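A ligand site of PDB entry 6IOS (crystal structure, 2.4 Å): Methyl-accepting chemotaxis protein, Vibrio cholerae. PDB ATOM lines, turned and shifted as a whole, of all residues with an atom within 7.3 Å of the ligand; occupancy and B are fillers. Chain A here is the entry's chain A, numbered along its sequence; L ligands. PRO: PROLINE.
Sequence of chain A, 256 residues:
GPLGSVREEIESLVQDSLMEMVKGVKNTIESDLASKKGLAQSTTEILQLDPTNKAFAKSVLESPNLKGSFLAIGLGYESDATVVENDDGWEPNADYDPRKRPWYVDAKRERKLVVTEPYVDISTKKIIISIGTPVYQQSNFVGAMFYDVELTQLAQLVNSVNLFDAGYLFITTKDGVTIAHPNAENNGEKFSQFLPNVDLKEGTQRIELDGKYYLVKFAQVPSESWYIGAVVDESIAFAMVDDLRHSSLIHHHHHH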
ATOM      1  N   LEU A  71      38.087  21.526 -18.258  1.00  0.00           N
ATOM      2  CA  LEU A  71      38.026  21.892 -16.861  1.00  0.00           C
ATOM      3  C   LEU A  71      37.704  20.663 -16.006  1.00  0.00           C
ATOM      4  O   LEU A  71      38.271  20.498 -14.947  1.00  0.00           O
ATOM      5  CB  LEU A  71      36.983  22.992 -16.651  1.00  0.00           C
ATOM      6  CG  LEU A  71      36.703  23.425 -15.215  1.00  0.00           C
ATOM      7  CD1 LEU A  71      37.969  23.937 -14.555  1.00  0.00           C
ATOM      8  CD2 LEU A  71      35.599  24.479 -15.170  1.00  0.00           C
ATOM      9  N   ALA A  72      36.793  19.821 -16.484  1.00  0.00           N
ATOM     10  CA  ALA A  72      36.354  18.646 -15.746  1.00  0.00           C
ATOM     11  C   ALA A  72      35.616  17.763 -16.719  1.00  0.00           C
ATOM     12  O   ALA A  72      35.020  18.268 -17.678  1.00  0.00           O
ATOM     13  CB  ALA A  72      35.445  19.028 -14.561  1.00  0.00           C
ATOM     14  N   ILE A  73      35.659  16.462 -16.485  1.00  0.00           N
ATOM     15  CA  ILE A  73      34.932  15.495 -17.315  1.00  0.00           C
ATOM     16  C   ILE A  73      34.239  14.499 -16.399  1.00  0.00           C
ATOM     17  O   ILE A  73      34.790  14.105 -15.367  1.00  0.00           O
ATOM     18  CB  ILE A  73      35.882  14.708 -18.289  1.00  0.00           C
ATOM     19  CG1 ILE A  73      36.814  15.649 -19.044  1.00  0.00           C
ATOM     20  CG2 ILE A  73      35.098  13.810 -19.258  1.00  0.00           C
ATOM     21  CD1 ILE A  73      37.851  14.934 -19.863  1.00  0.00           C
ATOM     22  N   GLY A  74      33.022  14.086 -16.772  1.00  0.00           N
ATOM     23  CA  GLY A  74      32.356  13.024 -16.061  1.00  0.00           C
ATOM     24  C   GLY A  74      31.239  12.331 -16.818  1.00  0.00           C
ATOM     25  O   GLY A  74      30.860  12.723 -17.924  1.00  0.00           O
ATOM     26  N   VAL A  83      27.651   9.174 -10.557  1.00  0.00           N
ATOM     27  CA  VAL A  83      28.565   9.979 -11.358  1.00  0.00           C
ATOM     28  C   VAL A  83      29.994   9.465 -11.277  1.00  0.00           C
ATOM     29  O   VAL A  83      30.553   9.345 -10.177  1.00  0.00           O
ATOM     30  CB  VAL A  83      28.594  11.445 -10.893  1.00  0.00           C
ATOM     31  CG1 VAL A  83      29.462  12.267 -11.825  1.00  0.00           C
ATOM     32  CG2 VAL A  83      27.196  12.008 -10.809  1.00  0.00           C
ATOM     33  N   GLU A  85      33.687  10.722 -12.316  1.00  0.00           N
ATOM     34  CA  GLU A  85      34.061  12.110 -12.532  1.00  0.00           C
ATOM     35  C   GLU A  85      35.529  12.407 -12.153  1.00  0.00           C
ATOM     36  O   GLU A  85      36.031  11.862 -11.183  1.00  0.00           O
ATOM     37  CB  GLU A  85      33.026  12.962 -11.756  1.00  0.00           C
ATOM     38  CG  GLU A  85      33.539  14.146 -11.079  1.00  0.00           C
ATOM     39  CD  GLU A  85      34.337  13.854  -9.822  1.00  0.00           C
ATOM     40  OE1 GLU A  85      34.099  12.863  -9.080  1.00  0.00           O
ATOM     41  OE2 GLU A  85      35.245  14.640  -9.625  1.00  0.00           O
ATOM     42  N   ASP A  87      37.032  15.453 -11.436  1.00  0.00           N
ATOM     43  CA  ASP A  87      37.240  16.728 -10.779  1.00  0.00           C
ATOM     44  C   ASP A  87      37.910  16.492  -9.422  1.00  0.00           C
ATOM     45  O   ASP A  87      37.315  15.918  -8.523  1.00  0.00           O
ATOM     46  CB  ASP A  87      35.897  17.464 -10.634  1.00  0.00           C
ATOM     47  CG  ASP A  87      36.021  18.875 -10.125  1.00  0.00           C
ATOM     48  OD1 ASP A  87      36.987  19.232  -9.391  1.00  0.00           O
ATOM     49  OD2 ASP A  87      35.132  19.694 -10.441  1.00  0.00           O
ATOM     50  N   TRP A  90      35.919  18.194  -6.320  1.00  0.00           N
ATOM     51  CA  TRP A  90      34.469  18.082  -6.236  1.00  0.00           C
ATOM     52  C   TRP A  90      33.937  16.650  -6.180  1.00  0.00           C
ATOM     53  O   TRP A  90      34.361  15.766  -6.952  1.00  0.00           O
ATOM     54  CB  TRP A  90      33.787  18.790  -7.409  1.00  0.00           C
ATOM     55  CG  TRP A  90      32.283  18.744  -7.274  1.00  0.00           C
ATOM     56  CD1 TRP A  90      31.507  19.548  -6.491  1.00  0.00           C
ATOM     57  CD2 TRP A  90      31.378  17.835  -7.924  1.00  0.00           C
ATOM     58  NE1 TRP A  90      30.189  19.200  -6.613  1.00  0.00           N
ATOM     59  CE2 TRP A  90      30.073  18.151  -7.489  1.00  0.00           C
ATOM     60  CE3 TRP A  90      31.540  16.804  -8.858  1.00  0.00           C
ATOM     61  CZ2 TRP A  90      28.946  17.482  -7.944  1.00  0.00           C
ATOM     62  CZ3 TRP A  90      30.425  16.128  -9.303  1.00  0.00           C
ATOM     63  CH2 TRP A  90      29.137  16.478  -8.844  1.00  0.00           C
ATOM     64  N   TYR A  96      22.722  16.165  -5.264  1.00  0.00           N
ATOM     65  CA  TYR A  96      23.102  16.178  -6.694  1.00  0.00           C
ATOM     66  C   TYR A  96      22.558  14.973  -7.419  1.00  0.00           C
ATOM     67  O   TYR A  96      22.818  13.852  -7.056  1.00  0.00           O
ATOM     68  CB  TYR A  96      24.617  16.211  -6.851  1.00  0.00           C
ATOM     69  CG  TYR A  96      25.086  16.366  -8.293  1.00  0.00           C
ATOM     70  CD1 TYR A  96      25.223  17.622  -8.856  1.00  0.00           C
ATOM     71  CD2 TYR A  96      25.425  15.260  -9.076  1.00  0.00           C
ATOM     72  CE1 TYR A  96      25.665  17.791 -10.149  1.00  0.00           C
ATOM     73  CE2 TYR A  96      25.864  15.424 -10.378  1.00  0.00           C
ATOM     74  CZ  TYR A  96      25.983  16.699 -10.907  1.00  0.00           C
ATOM     75  OH  TYR A  96      26.422  16.920 -12.188  1.00  0.00           O
ATOM     76  N   ASP A  97      21.811  15.236  -8.482  1.00  0.00           N
ATOM     77  CA  ASP A  97      21.344  14.207  -9.395  1.00  0.00           C
ATOM     78  C   ASP A  97      21.774  14.615 -10.797  1.00  0.00           C
ATOM     79  O   ASP A  97      21.268  15.608 -11.326  1.00  0.00           O
ATOM     80  CB  ASP A  97      19.829  14.065  -9.316  1.00  0.00           C
ATOM     81  CG  ASP A  97      19.289  12.955 -10.183  1.00  0.00           C
ATOM     82  OD1 ASP A  97      20.043  12.378 -10.994  1.00  0.00           O
ATOM     83  OD2 ASP A  97      18.082  12.657 -10.056  1.00  0.00           O
ATOM     84  N   PRO A  98      22.703  13.862 -11.409  1.00  0.00           N
ATOM     85  CA  PRO A  98      23.251  14.182 -12.737  1.00  0.00           C
ATOM     86  C   PRO A  98      22.172  14.377 -13.804  1.00  0.00           C
ATOM     87  O   PRO A  98      22.342  15.186 -14.714  1.00  0.00           O
ATOM     88  CB  PRO A  98      24.137  12.965 -13.073  1.00  0.00           C
ATOM     89  CG  PRO A  98      23.719  11.894 -12.109  1.00  0.00           C
ATOM     90  CD  PRO A  98      23.300  12.628 -10.864  1.00  0.00           C
ATOM     91  N   ARG A 101      20.700  17.853 -14.672  1.00  0.00           N
ATOM     92  CA  ARG A 101      21.641  18.878 -15.115  1.00  0.00           C
ATOM     93  C   ARG A 101      21.526  19.177 -16.622  1.00  0.00           C
ATOM     94  O   ARG A 101      21.104  18.327 -17.402  1.00  0.00           O
ATOM     95  CB  ARG A 101      23.080  18.451 -14.758  1.00  0.00           C
ATOM     96  CG  ARG A 101      23.307  18.233 -13.243  1.00  0.00           C
ATOM     97  CD  ARG A 101      23.093  19.521 -12.457  1.00  0.00           C
ATOM     98  NE  ARG A 101      24.182  20.476 -12.633  1.00  0.00           N
ATOM     99  CZ  ARG A 101      24.063  21.777 -12.406  1.00  0.00           C
ATOM    100  NH1 ARG A 101      22.908  22.263 -11.985  1.00  0.00           N
ATOM    101  NH2 ARG A 101      25.096  22.595 -12.575  1.00  0.00           N
ATOM    102  N   PRO A 102      21.894  20.398 -17.030  1.00  0.00           N
ATOM    103  CA  PRO A 102      21.739  20.808 -18.443  1.00  0.00           C
ATOM    104  C   PRO A 102      22.546  19.996 -19.474  1.00  0.00           C
ATOM    105  O   PRO A 102      21.971  19.679 -20.524  1.00  0.00           O
ATOM    106  CB  PRO A 102      22.183  22.284 -18.435  1.00  0.00           C
ATOM    107  CG  PRO A 102      22.687  22.581 -17.070  1.00  0.00           C
ATOM    108  CD  PRO A 102      22.197  21.523 -16.140  1.00  0.00           C
ATOM    109  N   TRP A 103      23.810  19.657 -19.203  1.00  0.00           N
ATOM    110  CA  TRP A 103      24.578  18.831 -20.138  1.00  0.00           C
ATOM    111  C   TRP A 103      23.867  17.503 -20.375  1.00  0.00           C
ATOM    112  O   TRP A 103      23.865  16.971 -21.476  1.00  0.00           O
ATOM    113  CB  TRP A 103      26.008  18.593 -19.619  1.00  0.00           C
ATOM    114  CG  TRP A 103      26.085  18.167 -18.165  1.00  0.00           C
ATOM    115  CD1 TRP A 103      26.140  18.985 -17.069  1.00  0.00           C
ATOM    116  CD2 TRP A 103      26.117  16.825 -17.645  1.00  0.00           C
ATOM    117  NE1 TRP A 103      26.218  18.257 -15.911  1.00  0.00           N
ATOM    118  CE2 TRP A 103      26.200  16.918 -16.240  1.00  0.00           C
ATOM    119  CE3 TRP A 103      26.112  15.550 -18.236  1.00  0.00           C
ATOM    120  CZ2 TRP A 103      26.264  15.782 -15.405  1.00  0.00           C
ATOM    121  CZ3 TRP A 103      26.165  14.422 -17.412  1.00  0.00           C
ATOM    122  CH2 TRP A 103      26.245  14.548 -16.009  1.00  0.00           C
ATOM    123  N   TYR A 119      25.804  28.074 -17.835  1.00  0.00           N
ATOM    124  CA  TYR A 119      25.067  27.795 -16.599  1.00  0.00           C
ATOM    125  C   TYR A 119      26.043  27.767 -15.450  1.00  0.00           C
ATOM    126  O   TYR A 119      27.253  27.742 -15.674  1.00  0.00           O
ATOM    127  CB  TYR A 119      24.315  26.469 -16.689  1.00  0.00           C
ATOM    128  CG  TYR A 119      25.213  25.244 -16.801  1.00  0.00           C
ATOM    129  CD1 TYR A 119      25.800  24.888 -18.002  1.00  0.00           C
ATOM    130  CD2 TYR A 119      25.469  24.435 -15.694  1.00  0.00           C
ATOM    131  CE1 TYR A 119      26.600  23.777 -18.114  1.00  0.00           C
ATOM    132  CE2 TYR A 119      26.270  23.309 -15.787  1.00  0.00           C
ATOM    133  CZ  TYR A 119      26.829  22.984 -17.003  1.00  0.00           C
ATOM    134  OH  TYR A 119      27.624  21.859 -17.118  1.00  0.00           O
ATOM    135  N   VAL A 120      25.517  27.757 -14.219  1.00  0.00           N
ATOM    136  CA  VAL A 120      26.375  27.751 -13.053  1.00  0.00           C
ATOM    137  C   VAL A 120      26.876  26.331 -12.734  1.00  0.00           C
ATOM    138  O   VAL A 120      26.095  25.403 -12.526  1.00  0.00           O
ATOM    139  CB  VAL A 120      25.676  28.312 -11.831  1.00  0.00           C
ATOM    140  CG1 VAL A 120      26.647  28.375 -10.639  1.00  0.00           C
ATOM    141  CG2 VAL A 120      25.097  29.683 -12.152  1.00  0.00           C
ATOM    142  N   ASP A 121      28.200  26.197 -12.730  1.00  0.00           N
ATOM    143  CA  ASP A 121      28.900  24.990 -12.373  1.00  0.00           C
ATOM    144  C   ASP A 121      28.692  24.672 -10.883  1.00  0.00           C
ATOM    145  O   ASP A 121      28.920  25.524 -10.033  1.00  0.00           O
ATOM    146  CB  ASP A 121      30.387  25.172 -12.684  1.00  0.00           C
ATOM    147  CG  ASP A 121      31.238  23.954 -12.316  1.00  0.00           C
ATOM    148  OD1 ASP A 121      30.678  22.867 -12.020  1.00  0.00           O
ATOM    149  OD2 ASP A 121      32.471  24.111 -12.339  1.00  0.00           O
ATOM    150  N   ILE A 122      28.273  23.451 -10.573  1.00  0.00           N
ATOM    151  CA  ILE A 122      28.080  23.121  -9.167  1.00  0.00           C
ATOM    152  C   ILE A 122      29.435  23.034  -8.461  1.00  0.00           C
ATOM    153  O   ILE A 122      29.554  23.304  -7.274  1.00  0.00           O
ATOM    154  CB  ILE A 122      27.280  21.815  -8.972  1.00  0.00           C
ATOM    155  CG1 ILE A 122      25.825  22.039  -9.415  1.00  0.00           C
ATOM    156  CG2 ILE A 122      27.245  21.422  -7.521  1.00  0.00           C
ATOM    157  CD1 ILE A 122      24.828  21.029  -8.848  1.00  0.00           C
ATOM    158  N   SER A 123      30.473  22.691  -9.220  1.00  0.00           N
ATOM    159  CA  SER A 123      31.791  22.586  -8.621  1.00  0.00           C
ATOM    160  C   SER A 123      32.437  23.963  -8.391  1.00  0.00           C
ATOM    161  O   SER A 123      32.691  24.357  -7.262  1.00  0.00           O
ATOM    162  CB  SER A 123      32.691  21.723  -9.513  1.00  0.00           C
ATOM    163  OG  SER A 123      34.022  21.699  -9.017  1.00  0.00           O
ATOM    164  N   THR A 124      32.726  24.702  -9.451  1.00  0.00           N
ATOM    165  CA  THR A 124      33.451  25.959  -9.281  1.00  0.00           C
ATOM    166  C   THR A 124      32.568  27.118  -8.882  1.00  0.00           C
ATOM    167  O   THR A 124      33.063  28.166  -8.466  1.00  0.00           O
ATOM    168  CB  THR A 124      34.217  26.350 -10.558  1.00  0.00           C
ATOM    169  OG1 THR A 124      33.297  26.509 -11.640  1.00  0.00           O
ATOM    170  CG2 THR A 124      35.274  25.264 -10.911  1.00  0.00           C
ATOM    171  N   ILE A 128      29.849  28.337 -16.649  1.00  0.00           N
ATOM    172  CA  ILE A 128      30.639  27.570 -17.598  1.00  0.00           C
ATOM    173  C   ILE A 128      29.775  27.215 -18.780  1.00  0.00           C
ATOM    174  O   ILE A 128      28.578  27.488 -18.775  1.00  0.00           O
ATOM    175  CB  ILE A 128      31.187  26.260 -16.972  1.00  0.00           C
ATOM    176  CG1 ILE A 128      30.034  25.420 -16.395  1.00  0.00           C
ATOM    177  CG2 ILE A 128      32.218  26.553 -15.892  1.00  0.00           C
ATOM    178  CD1 ILE A 128      30.396  23.933 -16.080  1.00  0.00           C
ATOM    179  N   SER A 130      29.417  23.437 -21.341  1.00  0.00           N
ATOM    180  CA  SER A 130      29.828  22.045 -21.378  1.00  0.00           C
ATOM    181  C   SER A 130      29.515  21.482 -22.733  1.00  0.00           C
ATOM    182  O   SER A 130      28.485  21.808 -23.325  1.00  0.00           O
ATOM    183  CB  SER A 130      29.113  21.189 -20.305  1.00  0.00           C
ATOM    184  OG  SER A 130      29.319  21.677 -18.986  1.00  0.00           O
ATOM    185  N   PHE A 146      29.616  14.950 -19.460  1.00  0.00           N
ATOM    186  CA  PHE A 146      29.942  16.372 -19.578  1.00  0.00           C
ATOM    187  C   PHE A 146      31.446  16.559 -19.768  1.00  0.00           C
ATOM    188  O   PHE A 146      32.257  15.812 -19.202  1.00  0.00           O
ATOM    189  CB  PHE A 146      29.479  17.159 -18.350  1.00  0.00           C
ATOM    190  CG  PHE A 146      30.147  16.736 -17.046  1.00  0.00           C
ATOM    191  CD1 PHE A 146      31.344  17.308 -16.633  1.00  0.00           C
ATOM    192  CD2 PHE A 146      29.540  15.797 -16.218  1.00  0.00           C
ATOM    193  CE1 PHE A 146      31.932  16.934 -15.425  1.00  0.00           C
ATOM    194  CE2 PHE A 146      30.124  15.411 -15.013  1.00  0.00           C
ATOM    195  CZ  PHE A 146      31.326  15.976 -14.612  1.00  0.00           C
ATOM    196  N   ASP A 148      33.491  19.987 -19.312  1.00  0.00           N
ATOM    197  CA  ASP A 148      33.340  21.381 -18.913  1.00  0.00           C
ATOM    198  C   ASP A 148      34.428  22.265 -19.530  1.00  0.00           C
ATOM    199  O   ASP A 148      35.588  21.878 -19.631  1.00  0.00           O
ATOM    200  CB  ASP A 148      33.365  21.522 -17.386  1.00  0.00           C
ATOM    201  CG  ASP A 148      32.167  20.878 -16.705  1.00  0.00           C
ATOM    202  OD1 ASP A 148      31.163  20.547 -17.375  1.00  0.00           O
ATOM    203  OD2 ASP A 148      32.244  20.744 -15.474  1.00  0.00           O
HETATM  204  N   PRO L   1      30.147  20.294 -13.726  1.00  0.00           N
HETATM  205  CA  PRO L   1      29.018  19.352 -13.729  1.00  0.00           C
HETATM  206  C   PRO L   1      27.721  19.961 -13.211  1.00  0.00           C
HETATM  207  O   PRO L   1      27.692  21.131 -12.782  1.00  0.00           O
HETATM  208  CB  PRO L   1      29.496  18.243 -12.800  1.00  0.00           C
HETATM  209  CG  PRO L   1      30.541  18.885 -11.916  1.00  0.00           C
HETATM  210  CD  PRO L   1      31.219  19.860 -12.792  1.00  0.00           C
HETATM  211  OXT PRO L   1      26.678  19.278 -13.197  1.00  0.00           O
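NE of Arg 101 lies within salt-bridge range of OXT of the ligand, at 2.8 Å. The backbone NH of Ile 122 is in hydrogen-bond range of an oxygen (O) of the ligand (3.3 Å). The indole nitrogen (NE1) of Trp 103 is in hydrogen-bond range of an oxygen (OXT) of the ligand. OD1 of Asp 121 is in salt-bridge range of N of the ligand. N of the ligand lies within salt-bridge range of OD2 of Asp 148 (2.8 Å). An oxygen (OXT) of the ligand sits at hydrogen-bond distance from the side-chain hydroxyl of Tyr 96 (2.6 Å).
NH2 of Arg 101 is in hydrogen-bond range of O of Val 120, at 3.0 Å. OG of Ser 130 lies within hydrogen-bond range of OH of Tyr 119 (2.5 Å). N of Ile 128 is in hydrogen-bond range of O of Tyr 119 (2.8 Å). O of Ala 72 lies within hydrogen-bond range of N of Asp 148. The backbone NH of Leu 71 is in hydrogen-bond range of the backbone carbonyl oxygen of Asp 148 (2.9 Å). OD1 of Asp 148 sits at hydrogen-bond distance from OG of Ser 130 (2.7 Å). The side-chain carboxylate (OD2) of Asp 121 lies within hydrogen-bond range of the side-chain hydroxyl (OG1) of Thr 124. N of Trp 90 lies within hydrogen-bond range of OD1 of Asp 87 (3.4 Å).
Trp 90 touches the ligand (CZ3 to CG, 3.8 Å). Tyr 119 touches the ligand (CE2 to O, 3.97 Å). Phe 146 touches the ligand (CZ to CB, 3.4 Å). Hydrophobic or aromatic side chains within 4 Å of the ligand: Trp 90, Tyr 96, Trp 103, Tyr 119, Ile 122 and Phe 146. Within 4 Å of the ligand: Trp 90, Tyr 96, Arg 101, Trp 103, Tyr 119, Asp 121, Ile 122, Phe 146 and Asp 148.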
